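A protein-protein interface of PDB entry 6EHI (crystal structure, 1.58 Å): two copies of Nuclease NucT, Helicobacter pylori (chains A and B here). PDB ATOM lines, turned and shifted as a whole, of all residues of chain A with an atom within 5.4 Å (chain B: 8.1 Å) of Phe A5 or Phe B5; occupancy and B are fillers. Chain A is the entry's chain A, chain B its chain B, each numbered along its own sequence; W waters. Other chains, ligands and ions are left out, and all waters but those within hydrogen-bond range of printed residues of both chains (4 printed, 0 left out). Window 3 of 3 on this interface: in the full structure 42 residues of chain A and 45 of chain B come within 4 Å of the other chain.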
ATOM      1  N   GLU A   4     -19.228  28.156  13.262  1.00  0.00           N
ATOM      2  CA  GLU A   4     -20.007  26.893  13.484  1.00  0.00           C
ATOM      3  C   GLU A   4     -19.435  25.921  14.532  1.00  0.00           C
ATOM      4  O   GLU A   4     -18.225  25.645  14.598  1.00  0.00           O
ATOM      5  CB  GLU A   4     -20.128  26.139  12.186  1.00  0.00           C
ATOM      6  CG  GLU A   4     -21.033  24.928  12.234  1.00  0.00           C
ATOM      7  CD  GLU A   4     -22.453  25.300  12.553  1.00  0.00           C
ATOM      8  OE1 GLU A   4     -22.744  26.514  12.520  1.00  0.00           O
ATOM      9  OE2 GLU A   4     -23.268  24.389  12.822  1.00  0.00           O
ATOM     10  N   PHE A   5     -20.342  25.364  15.310  1.00  0.00           N
ATOM     11  CA  PHE A   5     -19.966  24.490  16.401  1.00  0.00           C
ATOM     12  C   PHE A   5     -21.131  23.734  16.823  1.00  0.00           C
ATOM     13  O   PHE A   5     -22.228  24.042  16.462  1.00  0.00           O
ATOM     14  CB  PHE A   5     -19.398  25.316  17.596  1.00  0.00           C
ATOM     15  CG  PHE A   5     -20.381  26.296  18.236  1.00  0.00           C
ATOM     16  CD1 PHE A   5     -21.266  25.889  19.236  1.00  0.00           C
ATOM     17  CD2 PHE A   5     -20.367  27.644  17.859  1.00  0.00           C
ATOM     18  CE1 PHE A   5     -22.153  26.794  19.813  1.00  0.00           C
ATOM     19  CE2 PHE A   5     -21.228  28.557  18.465  1.00  0.00           C
ATOM     20  CZ  PHE A   5     -22.123  28.130  19.439  1.00  0.00           C
ATOM     21  N   LYS A   6     -20.892  22.789  17.708  1.00  0.00           N
ATOM     22  CA  LYS A   6     -21.913  21.958  18.202  1.00  0.00           C
ATOM     23  C   LYS A   6     -21.768  21.984  19.701  1.00  0.00           C
ATOM     24  O   LYS A   6     -20.673  21.644  20.183  1.00  0.00           O
ATOM     25  CB  LYS A   6     -21.633  20.560  17.670  1.00  0.00           C
ATOM     26  CG  LYS A   6     -22.397  19.430  18.336  1.00  0.00           C
ATOM     27  CD  LYS A   6     -23.868  19.457  18.076  1.00  0.00           C
ATOM     28  CE  LYS A   6     -24.465  18.078  18.444  1.00  0.00           C
ATOM     29  NZ  LYS A   6     -25.867  18.216  18.951  1.00  0.00           N
ATOM     30  N   ASN A   7     -22.811  22.453  20.370  1.00  0.00           N
ATOM     31  CA  ASN A   7     -22.985  22.275  21.811  1.00  0.00           C
ATOM     32  C   ASN A   7     -23.716  21.007  22.053  1.00  0.00           C
ATOM     33  O   ASN A   7     -24.785  20.745  21.479  1.00  0.00           O
ATOM     34  CB  ASN A   7     -23.687  23.463  22.452  1.00  0.00           C
ATOM     35  CG  ASN A   7     -22.799  24.666  22.604  1.00  0.00           C
ATOM     36  OD1 ASN A   7     -21.615  24.622  22.275  1.00  0.00           O
ATOM     37  ND2 ASN A   7     -23.386  25.804  23.008  1.00  0.00           N
ATOM     38  N   THR A 139     -18.513  21.055  24.106  1.00  0.00           N
ATOM     39  CA  THR A 139     -18.434  21.888  22.906  1.00  0.00           C
ATOM     40  C   THR A 139     -17.178  21.699  22.142  1.00  0.00           C
ATOM     41  O   THR A 139     -16.110  21.420  22.706  1.00  0.00           O
ATOM     42  CB  THR A 139     -18.714  23.366  23.189  1.00  0.00           C
ATOM     43  OG1 THR A 139     -18.790  24.130  21.959  1.00  0.00           O
ATOM     44  CG2 THR A 139     -17.650  23.978  24.013  1.00  0.00           C
ATOM     45  N   ASP A 140     -17.283  21.871  20.813  1.00  0.00           N
ATOM     46  CA  ASP A 140     -16.105  21.955  19.925  1.00  0.00           C
ATOM     47  C   ASP A 140     -15.858  23.377  19.401  1.00  0.00           C
ATOM     48  O   ASP A 140     -15.142  23.588  18.416  1.00  0.00           O
ATOM     49  CB  ASP A 140     -16.226  20.956  18.761  1.00  0.00           C
ATOM     50  CG  ASP A 140     -17.346  21.279  17.826  1.00  0.00           C
ATOM     51  OD1 ASP A 140     -18.109  22.234  18.069  1.00  0.00           O
ATOM     52  OD2 ASP A 140     -17.484  20.583  16.789  1.00  0.00           O
ATOM     53  N   ASP A 141     -16.459  24.383  20.028  1.00  0.00           N
ATOM     54  CA  ASP A 141     -16.294  25.734  19.623  1.00  0.00           C
ATOM     55  C   ASP A 141     -14.869  26.183  19.827  1.00  0.00           C
ATOM     56  O   ASP A 141     -14.364  26.251  20.972  1.00  0.00           O
ATOM     57  CB  ASP A 141     -17.224  26.616  20.444  1.00  0.00           C
ATOM     58  CG  ASP A 141     -17.123  28.070  20.093  1.00  0.00           C
ATOM     59  OD1 ASP A 141     -17.082  28.437  18.916  1.00  0.00           O
ATOM     60  OD2 ASP A 141     -17.115  28.883  21.005  1.00  0.00           O
ATOM     61  N   PHE B   5     -24.802  31.623  15.926  1.00  0.00           N
ATOM     62  CA  PHE B   5     -24.717  31.431  17.436  1.00  0.00           C
ATOM     63  C   PHE B   5     -23.347  31.670  18.035  1.00  0.00           C
ATOM     64  O   PHE B   5     -22.352  31.506  17.373  1.00  0.00           O
ATOM     65  CB  PHE B   5     -25.150  30.028  17.846  1.00  0.00           C
ATOM     66  CG  PHE B   5     -26.485  29.682  17.350  1.00  0.00           C
ATOM     67  CD1 PHE B   5     -27.566  30.482  17.685  1.00  0.00           C
ATOM     68  CD2 PHE B   5     -26.674  28.594  16.511  1.00  0.00           C
ATOM     69  CE1 PHE B   5     -28.817  30.172  17.240  1.00  0.00           C
ATOM     70  CE2 PHE B   5     -27.936  28.300  16.039  1.00  0.00           C
ATOM     71  CZ  PHE B   5     -29.003  29.095  16.406  1.00  0.00           C
ATOM     72  N   LYS B   6     -23.337  32.041  19.321  1.00  0.00           N
ATOM     73  CA  LYS B   6     -22.158  32.495  20.032  1.00  0.00           C
ATOM     74  C   LYS B   6     -22.112  31.785  21.416  1.00  0.00           C
ATOM     75  O   LYS B   6     -23.150  31.736  22.107  1.00  0.00           O
ATOM     76  CB  LYS B   6     -22.256  34.007  20.277  1.00  0.00           C
ATOM     77  CG  LYS B   6     -20.958  34.689  20.724  1.00  0.00           C
ATOM     78  CD  LYS B   6     -21.151  36.200  20.917  1.00  0.00           C
ATOM     79  CE  LYS B   6     -19.879  37.020  20.708  1.00  0.00           C
ATOM     80  NZ  LYS B   6     -19.541  37.303  19.267  1.00  0.00           N
ATOM     81  N   ASN B   7     -20.937  31.275  21.781  1.00  0.00           N
ATOM     82  CA  ASN B   7     -20.628  30.903  23.164  1.00  0.00           C
ATOM     83  C   ASN B   7     -19.674  31.953  23.695  1.00  0.00           C
ATOM     84  O   ASN B   7     -18.798  32.363  22.954  1.00  0.00           O
ATOM     85  CB  ASN B   7     -19.911  29.550  23.230  1.00  0.00           C
ATOM     86  CG  ASN B   7     -20.781  28.368  22.949  1.00  0.00           C
ATOM     87  OD1 ASN B   7     -22.020  28.369  23.128  1.00  0.00           O
ATOM     88  ND2 ASN B   7     -20.110  27.266  22.619  1.00  0.00           N
ATOM     89  N   SER B   8     -19.861  32.401  24.921  1.00  0.00           N
ATOM     90  CA  SER B   8     -18.999  33.362  25.573  1.00  0.00           C
ATOM     91  C   SER B   8     -18.556  32.706  26.886  1.00  0.00           C
ATOM     92  O   SER B   8     -19.365  32.517  27.818  1.00  0.00           O
ATOM     93  CB  SER B   8     -19.697  34.658  25.839  1.00  0.00           C
ATOM     94  OG  SER B   8     -20.118  35.201  24.588  1.00  0.00           O
ATOM     95  N   LYS B 115     -33.697  32.998  24.832  1.00  0.00           N
ATOM     96  CA  LYS B 115     -32.642  33.695  24.177  1.00  0.00           C
ATOM     97  C   LYS B 115     -31.243  33.354  24.698  1.00  0.00           C
ATOM     98  O   LYS B 115     -30.280  33.470  23.948  1.00  0.00           O
ATOM     99  CB  LYS B 115     -32.853  35.229  24.280  1.00  0.00           C
ATOM    100  CG  LYS B 115     -33.921  35.750  23.303  1.00  0.00           C
ATOM    101  CD  LYS B 115     -33.591  35.461  21.819  1.00  0.00           C
ATOM    102  CE  LYS B 115     -34.784  35.536  20.874  1.00  0.00           C
ATOM    103  NZ  LYS B 115     -35.559  36.792  21.048  1.00  0.00           N
ATOM    104  N   LEU B 137     -20.240  29.892  31.281  1.00  0.00           N
ATOM    105  CA  LEU B 137     -20.526  29.938  29.885  1.00  0.00           C
ATOM    106  C   LEU B 137     -21.927  30.571  29.634  1.00  0.00           C
ATOM    107  O   LEU B 137     -22.902  30.075  30.129  1.00  0.00           O
ATOM    108  CB  LEU B 137     -20.512  28.572  29.296  1.00  0.00           C
ATOM    109  CG  LEU B 137     -20.675  28.584  27.754  1.00  0.00           C
ATOM    110  CD1 LEU B 137     -19.380  28.824  27.078  1.00  0.00           C
ATOM    111  CD2 LEU B 137     -21.184  27.266  27.298  1.00  0.00           C
ATOM    112  N   LYS B 138     -21.971  31.579  28.755  1.00  0.00           N
ATOM    113  CA  LYS B 138     -23.202  32.167  28.219  1.00  0.00           C
ATOM    114  C   LYS B 138     -23.356  31.715  26.790  1.00  0.00           C
ATOM    115  O   LYS B 138     -22.399  31.797  25.999  1.00  0.00           O
ATOM    116  CB  LYS B 138     -23.114  33.710  28.212  1.00  0.00           C
ATOM    117  CG  LYS B 138     -24.249  34.469  27.562  1.00  0.00           C
ATOM    118  CD  LYS B 138     -24.006  35.975  27.550  1.00  0.00           C
ATOM    119  CE  LYS B 138     -25.098  36.657  26.741  1.00  0.00           C
ATOM    120  NZ  LYS B 138     -24.782  38.109  26.716  1.00  0.00           N
ATOM    121  N   THR B 139     -24.513  31.205  26.424  1.00  0.00           N
ATOM    122  CA  THR B 139     -24.755  30.767  25.042  1.00  0.00           C
ATOM    123  C   THR B 139     -26.139  31.218  24.533  1.00  0.00           C
ATOM    124  O   THR B 139     -27.089  31.268  25.293  1.00  0.00           O
ATOM    125  CB  THR B 139     -24.566  29.267  24.741  1.00  0.00           C
ATOM    126  OG1 THR B 139     -24.665  29.068  23.328  1.00  0.00           O
ATOM    127  CG2 THR B 139     -25.582  28.374  25.406  1.00  0.00           C
ATOM    128  N   ASP B 140     -26.208  31.620  23.259  1.00  0.00           N
ATOM    129  CA  ASP B 140     -27.472  31.826  22.576  1.00  0.00           C
ATOM    130  C   ASP B 140     -27.878  30.681  21.694  1.00  0.00           C
ATOM    131  O   ASP B 140     -28.797  30.795  20.913  1.00  0.00           O
ATOM    132  CB  ASP B 140     -27.505  33.198  21.856  1.00  0.00           C
ATOM    133  CG  ASP B 140     -26.490  33.319  20.735  1.00  0.00           C
ATOM    134  OD1 ASP B 140     -25.780  32.338  20.415  1.00  0.00           O
ATOM    135  OD2 ASP B 140     -26.371  34.450  20.196  1.00  0.00           O
ATOM    136  N   ASP B 141     -27.224  29.530  21.784  1.00  0.00           N
ATOM    137  CA  ASP B 141     -27.477  28.408  20.886  1.00  0.00           C
ATOM    138  C   ASP B 141     -28.865  27.841  21.072  1.00  0.00           C
ATOM    139  O   ASP B 141     -29.266  27.472  22.183  1.00  0.00           O
ATOM    140  CB  ASP B 141     -26.435  27.320  21.144  1.00  0.00           C
ATOM    141  CG  ASP B 141     -26.593  26.149  20.235  1.00  0.00           C
ATOM    142  OD1 ASP B 141     -26.427  26.371  19.032  1.00  0.00           O
ATOM    143  OD2 ASP B 141     -26.803  25.022  20.702  1.00  0.00           O
ATOM    144  N   THR B 142     -29.676  27.819  20.019  1.00  0.00           N
ATOM    145  CA  THR B 142     -31.084  27.505  20.238  1.00  0.00           C
ATOM    146  C   THR B 142     -31.331  26.090  20.721  1.00  0.00           C
ATOM    147  O   THR B 142     -32.201  25.894  21.572  1.00  0.00           O
ATOM    148  CB  THR B 142     -31.977  27.846  19.013  1.00  0.00           C
ATOM    149  OG1 THR B 142     -31.346  27.358  17.857  1.00  0.00           O
ATOM    150  CG2 THR B 142     -32.109  29.354  18.890  1.00  0.00           C
ATOM    151  N   GLU B 143     -30.579  25.118  20.221  1.00  0.00           N
ATOM    152  CA  GLU B 143     -30.810  23.735  20.613  1.00  0.00           C
ATOM    153  C   GLU B 143     -30.496  23.545  22.118  1.00  0.00           C
ATOM    154  O   GLU B 143     -31.234  22.860  22.835  1.00  0.00           O
ATOM    155  CB  GLU B 143     -29.937  22.826  19.759  1.00  0.00           C
ATOM    156  CG  GLU B 143     -29.921  21.335  20.134  1.00  0.00           C
ATOM    157  CD  GLU B 143     -28.664  20.589  19.636  1.00  0.00           C
ATOM    158  OE1 GLU B 143     -27.823  21.191  18.937  1.00  0.00           O
ATOM    159  OE2 GLU B 143     -28.486  19.390  19.971  1.00  0.00           O
ATOM    160  N   THR B 144     -29.391  24.170  22.559  1.00  0.00           N
ATOM    161  CA  THR B 144     -29.024  24.249  23.985  1.00  0.00           C
ATOM    162  C   THR B 144     -30.168  24.837  24.817  1.00  0.00           C
ATOM    163  O   THR B 144     -30.584  24.291  25.830  1.00  0.00           O
ATOM    164  CB  THR B 144     -27.708  25.017  24.176  1.00  0.00           C
ATOM    165  OG1 THR B 144     -26.698  24.435  23.376  1.00  0.00           O
ATOM    166  CG2 THR B 144     -27.202  24.983  25.662  1.00  0.00           C
ATOM    167  N   ILE B 145     -30.711  25.956  24.360  1.00  0.00           N
ATOM    168  CA  ILE B 145     -31.752  26.629  25.119  1.00  0.00           C
ATOM    169  C   ILE B 145     -33.010  25.767  25.193  1.00  0.00           C
ATOM    170  O   ILE B 145     -33.680  25.680  26.245  1.00  0.00           O
ATOM    171  CB  ILE B 145     -32.076  28.034  24.515  1.00  0.00           C
ATOM    172  CG1 ILE B 145     -30.879  28.981  24.688  1.00  0.00           C
ATOM    173  CG2 ILE B 145     -33.337  28.594  25.182  1.00  0.00           C
ATOM    174  CD1 ILE B 145     -30.878  30.226  23.812  1.00  0.00           C
HETATM  175  O   HOH W   1     -18.621  31.025  19.924  1.00  0.00           O
HETATM  176  O   HOH W   2     -25.321  23.144  19.026  1.00  0.00           O
HETATM  177  O   HOH W   3     -26.529  17.344  21.458  1.00  0.00           O
HETATM  178  O   HOH W   4     -26.917  21.758  22.839  1.00  0.00           O
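The side-chain amide nitrogen (ND2) of Asn A7 lies within hydrogen-bond range of the side-chain amide oxygen (OD1) of Asn B7 (2.9 Å).
NZ of Lys A6 lies within salt-bridge range of OE2 of Glu B143, 3.0 Å away.
The side-chain amide nitrogen (ND2) of Asn B7 lies within hydrogen-bond range of the side-chain hydroxyl (OG1) of Thr A139.
The side-chain amide oxygen of Asn A7 lies within hydrogen-bond range of the side-chain hydroxyl of Thr A139 (2.9 Å).
OD2 of Asp B141 sits at hydrogen-bond distance from OG1 of Thr B144 (2.7 Å).
N of Lys A6 sits at hydrogen-bond distance from OD1 of Asp A140 (2.9 Å).
The side-chain hydroxyl (OG1) of Thr A139 lies within hydrogen-bond range of the backbone NH (N) of Asp A141.
OG1 of Thr B139 is in hydrogen-bond range of N of Asp B141.
The side-chain hydroxyl of Thr B139 lies within hydrogen-bond range of the side-chain amide oxygen of Asn B7 (2.7 Å).
Among the printed residues, pairs that only touch across the chains: Asn A7 with Thr B144, Phe A5 with Phe B5, Phe A5 with Asn B7, Asn A7 with Thr B139, Asp A141 with Asn B7, Asn A7 with Asp B141 and Asn A7 with Glu B143.
Phe A5 touches just these residues of chain B: Phe B5 (3.3 Å) and Asn B7 (3.5 Å).
Of chain A, only Phe A5 (3.3 Å) comes within 4 Å of Phe B5.
No residue of chain B comes within 4 Å of Glu A4.
Printed residues of chain B within 4 Å of Thr A139: Asn B7 (3.5 Å).
Of the printed residues of chain B, Asn A7 touches Asn B7, Thr B139, Asp B141, Glu B143 and Thr B144.
Printed residues of chain A within 4 Å of Asn B7: Phe A5, Asn A7, Thr A139 and Asp A141.
Ile B145 touches none of the printed residues of chain A.
Of the 14 printed residues of chain B, 6 touch a printed residue of chain A.
Printed residues of chain B that touch a printed residue of chain A: Phe B5, Asn B7, Thr B139, Asp B141, Glu B143 and Thr B144.
Hydrophobic or aromatic side chains of chain B within 4 Å of the printed part of chain A: Phe B5.
Hydrophobic or aromatic side chains of chain A that line the printed part of chain B: Phe A5.
Along chain A the printed residues that touch a printed residue of chain B span positions 5 to 141.
Among the printed residues, 10 pairs touch across the chains.
Phe B5 touches its own counterpart, Phe A5.
Phe A5 touches Asn B7, but with the chains exchanged Asn A7 does not touch Phe B5 (6.9 Å).
Asn A7 touches its own counterpart, Asn B7.
Asn A7 touches Asp B141, and with the chains exchanged Asp A141 touches Asn B7.
Positions printed for both chains: 5, 6, 7, 139, 140 and 141.
Water W4 bridges the backbone carbonyl oxygen of Asn A7 (2.7 Å) and the side-chain hydroxyl of Thr B144 (2.7 Å).
Water W3 bridges NZ of Lys A6 (2.7 Å) and OE2 of Glu B143 (3.2 Å).
Water W1 lies within hydrogen-bond range of the side-chain carboxylate (OD2) of Asp A141 (2.8 Å) and the backbone NH (N) of Asn B7 (3.0 Å).
Water W2 lies within hydrogen-bond range of OD2 of Asp B141 (2.9 Å), N of Asn A7 (2.9 Å) and OE1 of Glu B143 (3.2 Å).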
